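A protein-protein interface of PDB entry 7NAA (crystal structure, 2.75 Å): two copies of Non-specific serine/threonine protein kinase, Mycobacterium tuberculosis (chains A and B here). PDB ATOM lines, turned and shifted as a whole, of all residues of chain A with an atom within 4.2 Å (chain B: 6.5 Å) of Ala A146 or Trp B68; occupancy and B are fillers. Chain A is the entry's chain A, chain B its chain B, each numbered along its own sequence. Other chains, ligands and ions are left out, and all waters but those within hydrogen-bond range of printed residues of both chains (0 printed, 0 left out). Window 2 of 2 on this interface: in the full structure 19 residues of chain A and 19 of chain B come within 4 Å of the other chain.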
ATOM      1  N   ASP A  90     -16.542 -18.195 -25.600  1.00  0.00           N
ATOM      2  CA  ASP A  90     -17.754 -18.317 -24.751  1.00  0.00           C
ATOM      3  C   ASP A  90     -18.740 -17.207 -25.107  1.00  0.00           C
ATOM      4  O   ASP A  90     -18.287 -16.089 -25.296  1.00  0.00           O
ATOM      5  CB  ASP A  90     -17.422 -18.151 -23.268  1.00  0.00           C
ATOM      6  CG  ASP A  90     -16.964 -19.406 -22.576  1.00  0.00           C
ATOM      7  OD1 ASP A  90     -17.328 -20.499 -23.062  1.00  0.00           O
ATOM      8  OD2 ASP A  90     -16.263 -19.250 -21.546  1.00  0.00           O
ATOM      9  N   VAL A  92     -21.600 -15.130 -23.305  1.00  0.00           N
ATOM     10  CA  VAL A  92     -22.133 -14.765 -21.965  1.00  0.00           C
ATOM     11  C   VAL A  92     -23.611 -14.398 -22.145  1.00  0.00           C
ATOM     12  O   VAL A  92     -23.921 -13.298 -22.610  1.00  0.00           O
ATOM     13  CB  VAL A  92     -21.322 -13.629 -21.333  1.00  0.00           C
ATOM     14  CG1 VAL A  92     -21.742 -13.365 -19.899  1.00  0.00           C
ATOM     15  CG2 VAL A  92     -19.834 -13.903 -21.397  1.00  0.00           C
ATOM     16  N   ASP A  93     -24.490 -15.336 -21.820  1.00  0.00           N
ATOM     17  CA  ASP A  93     -25.956 -15.216 -21.935  1.00  0.00           C
ATOM     18  C   ASP A  93     -26.474 -14.352 -20.783  1.00  0.00           C
ATOM     19  O   ASP A  93     -26.716 -14.883 -19.681  1.00  0.00           O
ATOM     20  CB  ASP A  93     -26.583 -16.604 -21.958  1.00  0.00           C
ATOM     21  CG  ASP A  93     -28.064 -16.597 -22.257  1.00  0.00           C
ATOM     22  OD1 ASP A  93     -28.569 -15.554 -22.776  1.00  0.00           O
ATOM     23  OD2 ASP A  93     -28.698 -17.639 -21.956  1.00  0.00           O
ATOM     24  N   GLY A  94     -26.617 -13.058 -21.070  1.00  0.00           N
ATOM     25  CA  GLY A  94     -27.134 -12.026 -20.155  1.00  0.00           C
ATOM     26  C   GLY A  94     -27.187 -10.680 -20.864  1.00  0.00           C
ATOM     27  O   GLY A  94     -27.722 -10.636 -21.981  1.00  0.00           O
ATOM     28  N   ILE A 145     -22.556  -9.509 -18.106  1.00  0.00           N
ATOM     29  CA  ILE A 145     -23.104 -10.092 -16.848  1.00  0.00           C
ATOM     30  C   ILE A 145     -24.111 -11.174 -17.236  1.00  0.00           C
ATOM     31  O   ILE A 145     -25.174 -10.827 -17.734  1.00  0.00           O
ATOM     32  CB  ILE A 145     -23.749  -9.015 -15.957  1.00  0.00           C
ATOM     33  CG1 ILE A 145     -22.815  -7.833 -15.717  1.00  0.00           C
ATOM     34  CG2 ILE A 145     -24.221  -9.629 -14.656  1.00  0.00           C
ATOM     35  CD1 ILE A 145     -23.398  -6.786 -14.801  1.00  0.00           C
ATOM     36  N   ALA A 146     -23.767 -12.447 -17.041  1.00  0.00           N
ATOM     37  CA  ALA A 146     -24.670 -13.595 -17.300  1.00  0.00           C
ATOM     38  C   ALA A 146     -25.634 -13.702 -16.119  1.00  0.00           C
ATOM     39  O   ALA A 146     -25.196 -13.420 -14.964  1.00  0.00           O
ATOM     40  CB  ALA A 146     -23.873 -14.852 -17.463  1.00  0.00           C
ATOM     41  N   ASN A 147     -26.896 -14.043 -16.395  1.00  0.00           N
ATOM     42  CA  ASN A 147     -27.946 -14.258 -15.357  1.00  0.00           C
ATOM     43  C   ASN A 147     -27.894 -13.100 -14.352  1.00  0.00           C
ATOM     44  O   ASN A 147     -27.660 -13.314 -13.159  1.00  0.00           O
ATOM     45  CB  ASN A 147     -27.780 -15.625 -14.679  1.00  0.00           C
ATOM     46  N   PRO A 148     -28.068 -11.836 -14.804  1.00  0.00           N
ATOM     47  CA  PRO A 148     -27.891 -10.675 -13.931  1.00  0.00           C
ATOM     48  C   PRO A 148     -28.776 -10.692 -12.679  1.00  0.00           C
ATOM     49  O   PRO A 148     -28.331 -10.207 -11.665  1.00  0.00           O
ATOM     50  CB  PRO A 148     -28.274  -9.476 -14.805  1.00  0.00           C
ATOM     51  CG  PRO A 148     -28.129  -9.967 -16.227  1.00  0.00           C
ATOM     52  CD  PRO A 148     -28.424 -11.453 -16.177  1.00  0.00           C
ATOM     53  N   ASP A 152     -26.881 -17.163  -9.981  1.00  0.00           N
ATOM     54  CA  ASP A 152     -25.806 -17.602 -10.915  1.00  0.00           C
ATOM     55  C   ASP A 152     -25.083 -16.394 -11.536  1.00  0.00           C
ATOM     56  O   ASP A 152     -24.268 -16.626 -12.449  1.00  0.00           O
ATOM     57  CB  ASP A 152     -26.387 -18.501 -12.015  1.00  0.00           C
ATOM     58  CG  ASP A 152     -26.688 -19.910 -11.558  1.00  0.00           C
ATOM     59  OD1 ASP A 152     -25.769 -20.546 -10.977  1.00  0.00           O
ATOM     60  OD2 ASP A 152     -27.825 -20.358 -11.794  1.00  0.00           O
ATOM     61  N   ARG A 153     -25.386 -15.173 -11.066  1.00  0.00           N
ATOM     62  CA  ARG A 153     -24.857 -13.875 -11.580  1.00  0.00           C
ATOM     63  C   ARG A 153     -23.337 -13.964 -11.722  1.00  0.00           C
ATOM     64  O   ARG A 153     -22.688 -14.407 -10.762  1.00  0.00           O
ATOM     65  CB  ARG A 153     -25.240 -12.751 -10.610  1.00  0.00           C
ATOM     66  CG  ARG A 153     -24.741 -11.363 -10.990  1.00  0.00           C
ATOM     67  CD  ARG A 153     -24.702 -10.429  -9.790  1.00  0.00           C
ATOM     68  NE  ARG A 153     -24.403  -9.070 -10.203  1.00  0.00           N
ATOM     69  CZ  ARG A 153     -25.300  -8.150 -10.571  1.00  0.00           C
ATOM     70  NH1 ARG A 153     -26.595  -8.429 -10.564  1.00  0.00           N
ATOM     71  NH2 ARG A 153     -24.884  -6.949 -10.934  1.00  0.00           N
ATOM     72  N   ARG A 154     -22.808 -13.547 -12.873  1.00  0.00           N
ATOM     73  CA  ARG A 154     -21.374 -13.690 -13.232  1.00  0.00           C
ATOM     74  C   ARG A 154     -20.955 -12.510 -14.118  1.00  0.00           C
ATOM     75  O   ARG A 154     -21.461 -12.427 -15.260  1.00  0.00           O
ATOM     76  CB  ARG A 154     -21.153 -15.009 -13.979  1.00  0.00           C
ATOM     77  CG  ARG A 154     -20.650 -16.162 -13.131  1.00  0.00           C
ATOM     78  CD  ARG A 154     -20.266 -17.320 -14.027  1.00  0.00           C
ATOM     79  NE  ARG A 154     -18.839 -17.334 -14.321  1.00  0.00           N
ATOM     80  CZ  ARG A 154     -18.240 -18.240 -15.079  1.00  0.00           C
ATOM     81  NH1 ARG A 154     -18.931 -19.204 -15.662  1.00  0.00           N
ATOM     82  NH2 ARG A 154     -16.939 -18.176 -15.269  1.00  0.00           N
ATOM     83  N   MET A 156     -18.197 -10.783 -16.476  1.00  0.00           N
ATOM     84  CA  MET A 156     -17.146 -11.254 -17.408  1.00  0.00           C
ATOM     85  C   MET A 156     -16.565 -10.065 -18.178  1.00  0.00           C
ATOM     86  O   MET A 156     -17.343  -9.175 -18.569  1.00  0.00           O
ATOM     87  CB  MET A 156     -17.725 -12.262 -18.399  1.00  0.00           C
ATOM     88  CG  MET A 156     -18.440 -13.432 -17.747  1.00  0.00           C
ATOM     89  SD  MET A 156     -17.406 -14.431 -16.642  1.00  0.00           S
ATOM     90  CE  MET A 156     -16.187 -15.027 -17.809  1.00  0.00           C
ATOM     91  N   ALA B  64     -21.802 -31.759 -21.186  1.00  0.00           N
ATOM     92  CA  ALA B  64     -20.579 -31.068 -20.706  1.00  0.00           C
ATOM     93  C   ALA B  64     -20.436 -29.680 -21.365  1.00  0.00           C
ATOM     94  O   ALA B  64     -20.039 -28.728 -20.648  1.00  0.00           O
ATOM     95  CB  ALA B  64     -19.377 -31.932 -20.988  1.00  0.00           C
ATOM     96  N   ALA B  65     -20.735 -29.576 -22.669  1.00  0.00           N
ATOM     97  CA  ALA B  65     -20.722 -28.322 -23.465  1.00  0.00           C
ATOM     98  C   ALA B  65     -21.893 -27.420 -23.059  1.00  0.00           C
ATOM     99  O   ALA B  65     -21.759 -26.195 -23.189  1.00  0.00           O
ATOM    100  CB  ALA B  65     -20.774 -28.640 -24.940  1.00  0.00           C
ATOM    101  N   SER B  66     -22.995 -28.020 -22.595  1.00  0.00           N
ATOM    102  CA  SER B  66     -24.204 -27.337 -22.057  1.00  0.00           C
ATOM    103  C   SER B  66     -23.866 -26.551 -20.781  1.00  0.00           C
ATOM    104  O   SER B  66     -24.561 -25.578 -20.495  1.00  0.00           O
ATOM    105  CB  SER B  66     -25.320 -28.331 -21.807  1.00  0.00           C
ATOM    106  N   LEU B  67     -22.857 -26.973 -20.013  1.00  0.00           N
ATOM    107  CA  LEU B  67     -22.552 -26.395 -18.677  1.00  0.00           C
ATOM    108  C   LEU B  67     -21.501 -25.296 -18.808  1.00  0.00           C
ATOM    109  O   LEU B  67     -20.497 -25.544 -19.464  1.00  0.00           O
ATOM    110  CB  LEU B  67     -22.082 -27.509 -17.740  1.00  0.00           C
ATOM    111  CG  LEU B  67     -23.145 -28.554 -17.397  1.00  0.00           C
ATOM    112  CD1 LEU B  67     -22.531 -29.740 -16.695  1.00  0.00           C
ATOM    113  CD2 LEU B  67     -24.257 -27.970 -16.555  1.00  0.00           C
ATOM    114  N   TRP B  68     -21.747 -24.144 -18.169  1.00  0.00           N
ATOM    115  CA  TRP B  68     -20.819 -22.982 -18.099  1.00  0.00           C
ATOM    116  C   TRP B  68     -20.744 -22.532 -16.636  1.00  0.00           C
ATOM    117  O   TRP B  68     -21.641 -21.797 -16.168  1.00  0.00           O
ATOM    118  CB  TRP B  68     -21.299 -21.882 -19.065  1.00  0.00           C
ATOM    119  CG  TRP B  68     -20.411 -20.679 -19.197  1.00  0.00           C
ATOM    120  CD1 TRP B  68     -19.247 -20.600 -19.897  1.00  0.00           C
ATOM    121  CD2 TRP B  68     -20.637 -19.363 -18.655  1.00  0.00           C
ATOM    122  NE1 TRP B  68     -18.716 -19.342 -19.813  1.00  0.00           N
ATOM    123  CE2 TRP B  68     -19.541 -18.562 -19.046  1.00  0.00           C
ATOM    124  CE3 TRP B  68     -21.636 -18.796 -17.854  1.00  0.00           C
ATOM    125  CZ2 TRP B  68     -19.427 -17.221 -18.669  1.00  0.00           C
ATOM    126  CZ3 TRP B  68     -21.508 -17.484 -17.461  1.00  0.00           C
ATOM    127  CH2 TRP B  68     -20.418 -16.709 -17.865  1.00  0.00           C
ATOM    128  N   HIS B  69     -19.731 -22.993 -15.918  1.00  0.00           N
ATOM    129  CA  HIS B  69     -19.561 -22.761 -14.459  1.00  0.00           C
ATOM    130  C   HIS B  69     -18.079 -22.593 -14.162  1.00  0.00           C
ATOM    131  O   HIS B  69     -17.254 -23.269 -14.777  1.00  0.00           O
ATOM    132  CB  HIS B  69     -20.209 -23.904 -13.662  1.00  0.00           C
ATOM    133  CG  HIS B  69     -20.422 -23.593 -12.223  1.00  0.00           C
ATOM    134  ND1 HIS B  69     -19.402 -23.684 -11.295  1.00  0.00           N
ATOM    135  CD2 HIS B  69     -21.520 -23.206 -11.547  1.00  0.00           C
ATOM    136  CE1 HIS B  69     -19.866 -23.342 -10.108  1.00  0.00           C
ATOM    137  NE2 HIS B  69     -21.165 -23.038 -10.238  1.00  0.00           N
ATOM    138  N   PRO B  70     -17.697 -21.676 -13.246  1.00  0.00           N
ATOM    139  CA  PRO B  70     -16.287 -21.442 -12.942  1.00  0.00           C
ATOM    140  C   PRO B  70     -15.571 -22.630 -12.278  1.00  0.00           C
ATOM    141  O   PRO B  70     -14.363 -22.604 -12.240  1.00  0.00           O
ATOM    142  CB  PRO B  70     -16.312 -20.228 -11.996  1.00  0.00           C
ATOM    143  CG  PRO B  70     -17.698 -20.204 -11.413  1.00  0.00           C
ATOM    144  CD  PRO B  70     -18.584 -20.788 -12.487  1.00  0.00           C
ATOM    145  N   ILE B  72     -16.569 -26.018 -13.107  1.00  0.00           N
ATOM    146  CA  ILE B  72     -16.752 -27.192 -14.019  1.00  0.00           C
ATOM    147  C   ILE B  72     -15.777 -27.019 -15.180  1.00  0.00           C
ATOM    148  O   ILE B  72     -15.759 -25.951 -15.760  1.00  0.00           O
ATOM    149  CB  ILE B  72     -18.213 -27.322 -14.503  1.00  0.00           C
ATOM    150  CG1 ILE B  72     -19.170 -27.532 -13.328  1.00  0.00           C
ATOM    151  CG2 ILE B  72     -18.364 -28.411 -15.550  1.00  0.00           C
ATOM    152  CD1 ILE B  72     -20.638 -27.553 -13.709  1.00  0.00           C
ATOM    153  N   ALA B  74     -14.300 -26.926 -18.740  1.00  0.00           N
ATOM    154  CA  ALA B  74     -14.971 -26.485 -19.984  1.00  0.00           C
ATOM    155  C   ALA B  74     -14.574 -27.398 -21.143  1.00  0.00           C
ATOM    156  O   ALA B  74     -13.387 -27.745 -21.218  1.00  0.00           O
ATOM    157  CB  ALA B  74     -14.576 -25.068 -20.282  1.00  0.00           C
ATOM    158  N   TYR B 127     -25.651 -26.467  -9.590  1.00  0.00           N
ATOM    159  CA  TYR B 127     -25.819 -25.772 -10.890  1.00  0.00           C
ATOM    160  C   TYR B 127     -26.255 -26.792 -11.953  1.00  0.00           C
ATOM    161  O   TYR B 127     -27.280 -26.563 -12.623  1.00  0.00           O
ATOM    162  CB  TYR B 127     -24.532 -25.027 -11.261  1.00  0.00           C
ATOM    163  CG  TYR B 127     -24.506 -24.453 -12.656  1.00  0.00           C
ATOM    164  CD1 TYR B 127     -24.051 -25.215 -13.719  1.00  0.00           C
ATOM    165  CD2 TYR B 127     -24.911 -23.155 -12.917  1.00  0.00           C
ATOM    166  CE1 TYR B 127     -24.018 -24.713 -15.009  1.00  0.00           C
ATOM    167  CE2 TYR B 127     -24.874 -22.631 -14.199  1.00  0.00           C
ATOM    168  CZ  TYR B 127     -24.434 -23.415 -15.256  1.00  0.00           C
ATOM    169  OH  TYR B 127     -24.391 -22.938 -16.542  1.00  0.00           O
ATOM    170  N   ARG B 131     -30.199 -27.729 -14.096  1.00  0.00           N
ATOM    171  CA  ARG B 131     -30.278 -27.913 -15.575  1.00  0.00           C
ATOM    172  C   ARG B 131     -30.505 -29.387 -15.943  1.00  0.00           C
ATOM    173  O   ARG B 131     -30.188 -29.762 -17.101  1.00  0.00           O
ATOM    174  CB  ARG B 131     -28.988 -27.393 -16.220  1.00  0.00           C
ATOM    175  CG  ARG B 131     -28.885 -25.878 -16.206  1.00  0.00           C
ATOM    176  CD  ARG B 131     -27.500 -25.334 -15.963  1.00  0.00           C
ATOM    177  NE  ARG B 131     -27.639 -23.897 -15.736  1.00  0.00           N
ATOM    178  CZ  ARG B 131     -28.040 -23.317 -14.593  1.00  0.00           C
ATOM    179  NH1 ARG B 131     -28.323 -24.043 -13.519  1.00  0.00           N
ATOM    180  NH2 ARG B 131     -28.138 -21.996 -14.530  1.00  0.00           N
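Ala A146 touches Trp B68. Asp A152 touches Tyr B127. Arg A154 touches Trp B68 (NH1 to CD2, 3.4 Å). Arg A154 touches His B69 (NH1 to C, 3.8 Å). NH1 of Arg A154 touches CD of Pro B70 (3.6 Å). Trp B68 touches Met A156.
The backbone NH (N) of Ala A146 sits at hydrogen-bond distance from the backbone carbonyl oxygen (O) of Arg A154 (2.9 Å). O of Trp B68 lies within hydrogen-bond range of OH of Tyr B127 (3.0 Å). O of Tyr B127 lies within hydrogen-bond range of NH1 of Arg B131 (2.9 Å).
No position is printed for both chains.
OD2 of Asp A90 is in hydrogen-bond range of NE1 of Trp B68 (3.0 Å). OD2 of Asp A152 is in salt-bridge range of NH2 of Arg B131 (3.2 Å).
Of the 12 printed residues of chain A, 5 touch a printed residue of chain B. Hydrophobic or aromatic side chains of chain A that line the printed part of chain B: Ala A146 and Met A156. Printed residues of chain B that touch a printed residue of chain A: Trp B68, His B69, Pro B70, Tyr B127 and Arg B131. Hydrophobic or aromatic side chains of chain B that line the printed part of chain A: Trp B68, Pro B70 and Tyr B127. Among the printed residues, Asp or Glu carboxylates within 4 Å of a Lys or Arg side-chain nitrogen of the other chain: Asp A152 with Arg B131 (3.2 Å).
Ala A146 touches one residue of chain B. Printed residues of chain B within 4 Å of Met A156: Trp B68 (3.8 Å). Ser B66 touches none of the printed residues of chain A. Trp B68 touches four residues of chain A. Of the printed residues of chain A, His B69 touches Arg A154 (3.8 Å). Ile B72 touches none of the printed residues of chain A. Of the printed residues of chain A, Tyr B127 touches Asp A152 (3.4 Å). Of the printed residues of chain A, Arg B131 touches Asp A152 (3.2 Å). The nearest printed residue of chain B that does not touch Ala A146 is Tyr B127 (8.2 Å). The nearest residue of chain A that does not touch Trp B68 is Val A92 (4.1 Å). The nearest printed residue of chain B that does not touch Arg A154 is Tyr B127 (6.7 Å).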
